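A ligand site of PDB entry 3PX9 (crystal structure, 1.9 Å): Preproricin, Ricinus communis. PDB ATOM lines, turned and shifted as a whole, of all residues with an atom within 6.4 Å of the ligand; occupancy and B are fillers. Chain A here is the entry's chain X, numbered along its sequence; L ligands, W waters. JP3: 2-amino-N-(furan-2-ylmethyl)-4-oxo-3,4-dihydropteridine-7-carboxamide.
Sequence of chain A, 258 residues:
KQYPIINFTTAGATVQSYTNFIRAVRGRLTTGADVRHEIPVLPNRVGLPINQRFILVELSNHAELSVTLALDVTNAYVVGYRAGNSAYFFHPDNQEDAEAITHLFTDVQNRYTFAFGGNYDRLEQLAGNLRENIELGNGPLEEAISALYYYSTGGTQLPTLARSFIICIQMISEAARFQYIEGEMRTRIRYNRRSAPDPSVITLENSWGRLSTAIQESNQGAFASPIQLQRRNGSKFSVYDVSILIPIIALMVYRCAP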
ATOM      1  N   ASN A  75       7.540  31.089 -31.211  1.00  0.00           N
ATOM      2  CA  ASN A  75       7.406  29.693 -30.770  1.00  0.00           C
ATOM      3  C   ASN A  75       6.607  28.775 -31.736  1.00  0.00           C
ATOM      4  O   ASN A  75       6.289  27.646 -31.436  1.00  0.00           O
ATOM      5  CB  ASN A  75       6.711  29.681 -29.376  1.00  0.00           C
ATOM      6  CG  ASN A  75       5.352  30.438 -29.383  1.00  0.00           C
ATOM      7  OD1 ASN A  75       4.823  30.811 -30.426  1.00  0.00           O
ATOM      8  ND2 ASN A  75       4.828  30.676 -28.201  1.00  0.00           N
ATOM      9  N   ALA A  76       6.280  29.318 -32.867  1.00  0.00           N
ATOM     10  CA  ALA A  76       5.449  28.734 -33.912  1.00  0.00           C
ATOM     11  C   ALA A  76       4.020  28.424 -33.463  1.00  0.00           C
ATOM     12  O   ALA A  76       3.312  27.718 -34.189  1.00  0.00           O
ATOM     13  CB  ALA A  76       6.158  27.482 -34.613  1.00  0.00           C
ATOM     14  N   TYR A  77       3.575  28.967 -32.298  1.00  0.00           N
ATOM     15  CA  TYR A  77       2.185  28.707 -31.829  1.00  0.00           C
ATOM     16  C   TYR A  77       1.131  29.302 -32.744  1.00  0.00           C
ATOM     17  O   TYR A  77       1.237  30.411 -33.284  1.00  0.00           O
ATOM     18  CB  TYR A  77       1.930  29.146 -30.328  1.00  0.00           C
ATOM     19  CG  TYR A  77       2.253  28.109 -29.359  1.00  0.00           C
ATOM     20  CD1 TYR A  77       1.352  27.658 -28.424  1.00  0.00           C
ATOM     21  CD2 TYR A  77       3.575  27.578 -29.325  1.00  0.00           C
ATOM     22  CE1 TYR A  77       1.742  26.651 -27.490  1.00  0.00           C
ATOM     23  CE2 TYR A  77       3.966  26.609 -28.430  1.00  0.00           C
ATOM     24  CZ  TYR A  77       3.047  26.108 -27.539  1.00  0.00           C
ATOM     25  OH  TYR A  77       3.478  25.144 -26.631  1.00  0.00           O
ATOM     26  N   VAL A  78       0.083  28.516 -32.987  1.00  0.00           N
ATOM     27  CA  VAL A  78      -1.099  29.049 -33.620  1.00  0.00           C
ATOM     28  C   VAL A  78      -1.875  29.827 -32.566  1.00  0.00           C
ATOM     29  O   VAL A  78      -2.356  29.280 -31.550  1.00  0.00           O
ATOM     30  CB  VAL A  78      -1.953  27.915 -34.233  1.00  0.00           C
ATOM     31  CG1 VAL A  78      -3.210  28.474 -34.992  1.00  0.00           C
ATOM     32  CG2 VAL A  78      -1.097  27.053 -35.200  1.00  0.00           C
ATOM     33  N   VAL A  79      -2.059  31.109 -32.832  1.00  0.00           N
ATOM     34  CA  VAL A  79      -2.670  31.979 -31.817  1.00  0.00           C
ATOM     35  C   VAL A  79      -4.104  32.327 -32.126  1.00  0.00           C
ATOM     36  O   VAL A  79      -4.836  32.772 -31.262  1.00  0.00           O
ATOM     37  CB  VAL A  79      -1.862  33.291 -31.572  1.00  0.00           C
ATOM     38  CG1 VAL A  79      -0.439  32.971 -31.054  1.00  0.00           C
ATOM     39  CG2 VAL A  79      -1.824  34.186 -32.793  1.00  0.00           C
ATOM     40  N   PHE A  90      -7.240  32.330 -29.476  1.00  0.00           N
ATOM     41  CA  PHE A  90      -7.218  31.674 -28.165  1.00  0.00           C
ATOM     42  C   PHE A  90      -7.031  32.696 -27.041  1.00  0.00           C
ATOM     43  O   PHE A  90      -6.458  33.821 -27.245  1.00  0.00           O
ATOM     44  CB  PHE A  90      -6.112  30.640 -28.096  1.00  0.00           C
ATOM     45  CG  PHE A  90      -6.261  29.553 -29.083  1.00  0.00           C
ATOM     46  CD1 PHE A  90      -7.281  28.631 -28.965  1.00  0.00           C
ATOM     47  CD2 PHE A  90      -5.417  29.476 -30.186  1.00  0.00           C
ATOM     48  CE1 PHE A  90      -7.453  27.687 -29.889  1.00  0.00           C
ATOM     49  CE2 PHE A  90      -5.536  28.476 -31.092  1.00  0.00           C
ATOM     50  CZ  PHE A  90      -6.565  27.572 -30.952  1.00  0.00           C
ATOM     51  N   GLY A 118      -5.155  27.910 -26.026  1.00  0.00           N
ATOM     52  CA  GLY A 118      -4.825  27.006 -27.180  1.00  0.00           C
ATOM     53  C   GLY A 118      -3.853  25.801 -26.997  1.00  0.00           C
ATOM     54  O   GLY A 118      -3.441  25.197 -27.989  1.00  0.00           O
ATOM     55  N   ASN A 119      -3.421  25.496 -25.752  1.00  0.00           N
ATOM     56  CA  ASN A 119      -2.549  24.336 -25.511  1.00  0.00           C
ATOM     57  C   ASN A 119      -3.249  22.996 -25.800  1.00  0.00           C
ATOM     58  O   ASN A 119      -4.492  22.911 -25.764  1.00  0.00           O
ATOM     59  CB  ASN A 119      -2.010  24.341 -24.050  1.00  0.00           C
ATOM     60  CG  ASN A 119      -1.044  25.508 -23.794  1.00  0.00           C
ATOM     61  OD1 ASN A 119      -0.515  26.110 -24.726  1.00  0.00           O
ATOM     62  ND2 ASN A 119      -0.850  25.850 -22.514  1.00  0.00           N
ATOM     63  N   TYR A 120      -2.474  21.940 -26.111  1.00  0.00           N
ATOM     64  CA  TYR A 120      -3.076  20.646 -26.422  1.00  0.00           C
ATOM     65  C   TYR A 120      -3.975  20.179 -25.280  1.00  0.00           C
ATOM     66  O   TYR A 120      -4.988  19.562 -25.560  1.00  0.00           O
ATOM     67  CB  TYR A 120      -2.025  19.569 -26.654  1.00  0.00           C
ATOM     68  CG  TYR A 120      -1.198  19.697 -27.972  1.00  0.00           C
ATOM     69  CD1 TYR A 120      -1.813  20.014 -29.185  1.00  0.00           C
ATOM     70  CD2 TYR A 120       0.164  19.402 -27.992  1.00  0.00           C
ATOM     71  CE1 TYR A 120      -1.073  20.149 -30.377  1.00  0.00           C
ATOM     72  CE2 TYR A 120       0.914  19.500 -29.222  1.00  0.00           C
ATOM     73  CZ  TYR A 120       0.293  19.857 -30.389  1.00  0.00           C
ATOM     74  OH  TYR A 120       1.087  19.952 -31.546  1.00  0.00           O
ATOM     75  N   ASP A 121      -3.609  20.407 -24.019  1.00  0.00           N
ATOM     76  CA  ASP A 121      -4.391  19.883 -22.915  1.00  0.00           C
ATOM     77  C   ASP A 121      -5.807  20.373 -22.919  1.00  0.00           C
ATOM     78  O   ASP A 121      -6.752  19.604 -22.792  1.00  0.00           O
ATOM     79  CB  ASP A 121      -3.699  19.999 -21.529  1.00  0.00           C
ATOM     80  CG  ASP A 121      -3.085  21.370 -21.243  1.00  0.00           C
ATOM     81  OD1 ASP A 121      -3.370  22.346 -21.957  1.00  0.00           O
ATOM     82  OD2 ASP A 121      -2.317  21.454 -20.267  1.00  0.00           O
ATOM     83  N   LEU A 123      -7.363  21.840 -25.601  1.00  0.00           N
ATOM     84  CA  LEU A 123      -7.987  21.443 -26.827  1.00  0.00           C
ATOM     85  C   LEU A 123      -8.479  19.960 -26.799  1.00  0.00           C
ATOM     86  O   LEU A 123      -9.518  19.634 -27.323  1.00  0.00           O
ATOM     87  CB  LEU A 123      -7.068  21.690 -28.037  1.00  0.00           C
ATOM     88  CG  LEU A 123      -6.708  23.163 -28.255  1.00  0.00           C
ATOM     89  CD1 LEU A 123      -5.812  23.352 -29.419  1.00  0.00           C
ATOM     90  CD2 LEU A 123      -7.901  24.029 -28.477  1.00  0.00           C
ATOM     91  N   ARG A 131      -4.699  13.509 -28.689  1.00  0.00           N
ATOM     92  CA  ARG A 131      -3.975  13.465 -29.898  1.00  0.00           C
ATOM     93  C   ARG A 131      -3.742  12.013 -30.343  1.00  0.00           C
ATOM     94  O   ARG A 131      -3.683  11.739 -31.532  1.00  0.00           O
ATOM     95  CB  ARG A 131      -2.603  14.163 -29.717  1.00  0.00           C
ATOM     96  CG  ARG A 131      -2.630  15.650 -29.787  1.00  0.00           C
ATOM     97  CD  ARG A 131      -1.287  16.165 -29.305  1.00  0.00           C
ATOM     98  NE  ARG A 131      -1.100  16.035 -27.858  1.00  0.00           N
ATOM     99  CZ  ARG A 131       0.078  16.161 -27.243  1.00  0.00           C
ATOM    100  NH1 ARG A 131       1.207  16.306 -27.973  1.00  0.00           N
ATOM    101  NH2 ARG A 131       0.140  16.134 -25.891  1.00  0.00           N
ATOM    102  N   ILE A 169      -2.428  22.270 -35.990  1.00  0.00           N
ATOM    103  CA  ILE A 169      -1.244  22.567 -35.159  1.00  0.00           C
ATOM    104  C   ILE A 169      -0.161  21.529 -35.483  1.00  0.00           C
ATOM    105  O   ILE A 169       0.976  21.864 -35.729  1.00  0.00           O
ATOM    106  CB  ILE A 169      -1.560  22.653 -33.655  1.00  0.00           C
ATOM    107  CG1 ILE A 169      -2.452  23.859 -33.342  1.00  0.00           C
ATOM    108  CG2 ILE A 169      -0.289  22.720 -32.862  1.00  0.00           C
ATOM    109  CD1 ILE A 169      -3.043  23.774 -31.913  1.00  0.00           C
ATOM    110  N   SER A 173       2.583  23.671 -37.375  1.00  0.00           N
ATOM    111  CA  SER A 173       3.617  24.012 -36.376  1.00  0.00           C
ATOM    112  C   SER A 173       4.586  22.889 -35.985  1.00  0.00           C
ATOM    113  O   SER A 173       5.796  23.083 -35.964  1.00  0.00           O
ATOM    114  CB  SER A 173       2.974  24.571 -35.114  1.00  0.00           C
ATOM    115  OG  SER A 173       2.121  25.651 -35.478  1.00  0.00           O
ATOM    116  N   GLU A 174       4.071  21.733 -35.643  1.00  0.00           N
ATOM    117  CA  GLU A 174       4.910  20.624 -35.298  1.00  0.00           C
ATOM    118  C   GLU A 174       5.770  20.140 -36.452  1.00  0.00           C
ATOM    119  O   GLU A 174       6.964  19.817 -36.242  1.00  0.00           O
ATOM    120  CB  GLU A 174       4.066  19.482 -34.754  1.00  0.00           C
ATOM    121  CG  GLU A 174       3.277  19.770 -33.416  1.00  0.00           C
ATOM    122  CD  GLU A 174       4.116  20.142 -32.173  1.00  0.00           C
ATOM    123  OE1 GLU A 174       5.324  20.273 -32.257  1.00  0.00           O
ATOM    124  OE2 GLU A 174       3.509  20.251 -31.099  1.00  0.00           O
ATOM    125  N   ARG A 177       8.566  22.545 -36.635  1.00  0.00           N
ATOM    126  CA  ARG A 177       9.500  22.313 -35.537  1.00  0.00           C
ATOM    127  C   ARG A 177      10.381  21.131 -35.734  1.00  0.00           C
ATOM    128  O   ARG A 177      11.567  21.168 -35.316  1.00  0.00           O
ATOM    129  CB  ARG A 177       8.762  22.146 -34.179  1.00  0.00           C
ATOM    130  CG  ARG A 177       8.115  23.411 -33.718  1.00  0.00           C
ATOM    131  CD  ARG A 177       7.258  23.120 -32.404  1.00  0.00           C
ATOM    132  NE  ARG A 177       6.455  24.309 -32.108  1.00  0.00           N
ATOM    133  CZ  ARG A 177       5.160  24.292 -31.844  1.00  0.00           C
ATOM    134  NH1 ARG A 177       4.492  23.143 -31.867  1.00  0.00           N
ATOM    135  NH2 ARG A 177       4.525  25.447 -31.609  1.00  0.00           N
ATOM    136  N   GLU A 205       6.616  16.121 -29.705  1.00  0.00           N
ATOM    137  CA  GLU A 205       5.769  17.322 -29.487  1.00  0.00           C
ATOM    138  C   GLU A 205       5.828  17.831 -28.057  1.00  0.00           C
ATOM    139  O   GLU A 205       6.033  19.021 -27.844  1.00  0.00           O
ATOM    140  CB  GLU A 205       4.317  17.031 -29.809  1.00  0.00           C
ATOM    141  CG  GLU A 205       4.038  16.802 -31.294  1.00  0.00           C
ATOM    142  CD  GLU A 205       2.630  16.325 -31.542  1.00  0.00           C
ATOM    143  OE1 GLU A 205       1.857  16.172 -30.589  1.00  0.00           O
ATOM    144  OE2 GLU A 205       2.308  16.131 -32.719  1.00  0.00           O
ATOM    145  N   ASN A 206       5.654  16.917 -27.128  1.00  0.00           N
ATOM    146  CA  ASN A 206       5.637  17.207 -25.705  1.00  0.00           C
ATOM    147  C   ASN A 206       6.979  17.675 -25.179  1.00  0.00           C
ATOM    148  O   ASN A 206       7.041  18.432 -24.207  1.00  0.00           O
ATOM    149  CB  ASN A 206       5.221  15.960 -24.912  1.00  0.00           C
ATOM    150  CG  ASN A 206       3.744  15.615 -25.070  1.00  0.00           C
ATOM    151  OD1 ASN A 206       2.944  16.422 -25.555  1.00  0.00           O
ATOM    152  ND2 ASN A 206       3.368  14.389 -24.689  1.00  0.00           N
ATOM    153  N   SER A 207       8.045  17.242 -25.875  1.00  0.00           N
ATOM    154  CA  SER A 207       9.434  17.505 -25.461  1.00  0.00           C
ATOM    155  C   SER A 207      10.101  18.634 -26.145  1.00  0.00           C
ATOM    156  O   SER A 207      11.282  18.842 -25.924  1.00  0.00           O
ATOM    157  CB  SER A 207      10.290  16.276 -25.721  1.00  0.00           C
ATOM    158  OG  SER A 207       9.688  15.114 -25.176  1.00  0.00           O
ATOM    159  N   TRP A 208       9.385  19.413 -26.975  1.00  0.00           N
ATOM    160  CA  TRP A 208      10.017  20.453 -27.750  1.00  0.00           C
ATOM    161  C   TRP A 208      10.708  21.506 -26.877  1.00  0.00           C
ATOM    162  O   TRP A 208      11.889  21.943 -27.139  1.00  0.00           O
ATOM    163  CB  TRP A 208       9.051  21.148 -28.656  1.00  0.00           C
ATOM    164  CG  TRP A 208       9.694  22.129 -29.581  1.00  0.00           C
ATOM    165  CD1 TRP A 208      10.667  21.847 -30.467  1.00  0.00           C
ATOM    166  CD2 TRP A 208       9.374  23.514 -29.745  1.00  0.00           C
ATOM    167  NE1 TRP A 208      10.976  22.958 -31.197  1.00  0.00           N
ATOM    168  CE2 TRP A 208      10.200  23.998 -30.760  1.00  0.00           C
ATOM    169  CE3 TRP A 208       8.437  24.378 -29.154  1.00  0.00           C
ATOM    170  CZ2 TRP A 208      10.183  25.331 -31.169  1.00  0.00           C
ATOM    171  CZ3 TRP A 208       8.433  25.693 -29.527  1.00  0.00           C
ATOM    172  CH2 TRP A 208       9.228  26.151 -30.552  1.00  0.00           C
ATOM    173  N   GLY A 209      10.015  21.968 -25.861  1.00  0.00           N
ATOM    174  CA  GLY A 209      10.661  22.994 -24.978  1.00  0.00           C
ATOM    175  C   GLY A 209      11.842  22.419 -24.232  1.00  0.00           C
ATOM    176  O   GLY A 209      12.915  23.038 -24.140  1.00  0.00           O
HETATM  177  C1  JP3 L   1      -1.150  25.969 -30.277  1.00  0.00           C
HETATM  178  N1  JP3 L   1      -2.254  26.712 -30.376  1.00  0.00           N
HETATM  179  O1  JP3 L   1       1.827  25.466 -31.954  1.00  0.00           O
HETATM  180  C2  JP3 L   1       0.946  25.348 -31.102  1.00  0.00           C
HETATM  181  N2  JP3 L   1      -0.171  26.117 -31.216  1.00  0.00           N
HETATM  182  O2  JP3 L   1       0.461  21.918 -25.829  1.00  0.00           O
HETATM  183  C3  JP3 L   1       1.097  24.402 -29.983  1.00  0.00           C
HETATM  184  N3  JP3 L   1      -1.075  25.110 -29.237  1.00  0.00           N
HETATM  185  O3  JP3 L   1       3.363  22.376 -23.449  1.00  0.00           O
HETATM  186  C4  JP3 L   1       0.001  24.330 -29.012  1.00  0.00           C
HETATM  187  N4  JP3 L   1       0.094  23.494 -27.967  1.00  0.00           N
HETATM  188  C5  JP3 L   1       1.237  22.746 -27.827  1.00  0.00           C
HETATM  189  N5  JP3 L   1       2.174  23.624 -29.808  1.00  0.00           N
HETATM  190  C6  JP3 L   1       2.279  22.827 -28.748  1.00  0.00           C
HETATM  191  N6  JP3 L   1       2.563  21.370 -26.279  1.00  0.00           N
HETATM  192  C7  JP3 L   1       1.400  21.935 -26.612  1.00  0.00           C
HETATM  193  C8  JP3 L   1       2.672  20.452 -25.115  1.00  0.00           C
HETATM  194  C9  JP3 L   1       3.498  21.074 -23.974  1.00  0.00           C
HETATM  195  C10 JP3 L   1       4.527  20.429 -23.241  1.00  0.00           C
HETATM  196  C11 JP3 L   1       4.999  21.354 -22.311  1.00  0.00           C
HETATM  197  C12 JP3 L   1       4.300  22.552 -22.430  1.00  0.00           C
HETATM  198  O   HOH W   1      -0.734  21.169 -23.489  1.00  0.00           O
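Ala 76 touches the ligand (O to O1, 3.5 Å). Tyr 77 touches the ligand (CA to O1, 3.3 Å). Phe 90 touches the ligand. Asn 119 touches the ligand. Ile 169 touches the ligand (CD1 to C1, 3.3 Å). CB of Ser 173 touches O1 of the ligand (3.5 Å). OE2 of Glu 174 touches C6 of the ligand, at 3.7 Å. Asn 206 touches the ligand (O to C10, 3.4 Å). 12 residues have an atom within 4 Å of the ligand: Ala 76, Tyr 77, Val 78, Phe 90, Gly 118, Asn 119, Tyr 120, Ile 169, Ser 173, Glu 174, Arg 177 and Asn 206. The nearest printed residue that does not touch the ligand is Glu 205 (4.5 Å).
The guanidinium group (NH1) of Arg 177 is in salt-bridge range of the side-chain carboxylate (OE1) of Glu 174. The backbone carbonyl oxygen (O) of Ile 169 sits at hydrogen-bond distance from the backbone NH (N) of Glu 174 (3.1 Å). OH of Tyr 120 is in hydrogen-bond range of OE2 of Glu 174. NH2 of Arg 131 lies within hydrogen-bond range of OD1 of Asn 206, at 2.8 Å. The backbone NH (N) of Tyr 77 lies within hydrogen-bond range of the side-chain amide oxygen (OD1) of Asn 75 (2.9 Å). The backbone NH (N) of Phe 90 is in hydrogen-bond range of the backbone carbonyl oxygen (O) of Val 79. The guanidinium group of Arg 177 sits at hydrogen-bond distance from the backbone carbonyl oxygen of Asn 75 (2.8 Å). The side-chain hydroxyl (OG) of Ser 173 lies within hydrogen-bond range of the backbone carbonyl oxygen (O) of Ala 76, at 2.7 Å.
The backbone carbonyl oxygen (O) of Gly 118 is in hydrogen-bond range of a nitrogen (N1) of the ligand (3.1 Å). NH2 of Arg 177 lies within hydrogen-bond range of O1 of the ligand (2.7 Å). N of Tyr 120 lies within hydrogen-bond range of O2 of the ligand (2.9 Å). A nitrogen (N1) of the ligand is in hydrogen-bond range of the backbone carbonyl oxygen of Val 78.
Water W1 lies within hydrogen-bond range of an oxygen (O2) of the ligand (2.7 Å), the backbone NH of Asp 121 (3.0 Å) and the backbone NH of Tyr 120 (3.2 Å).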
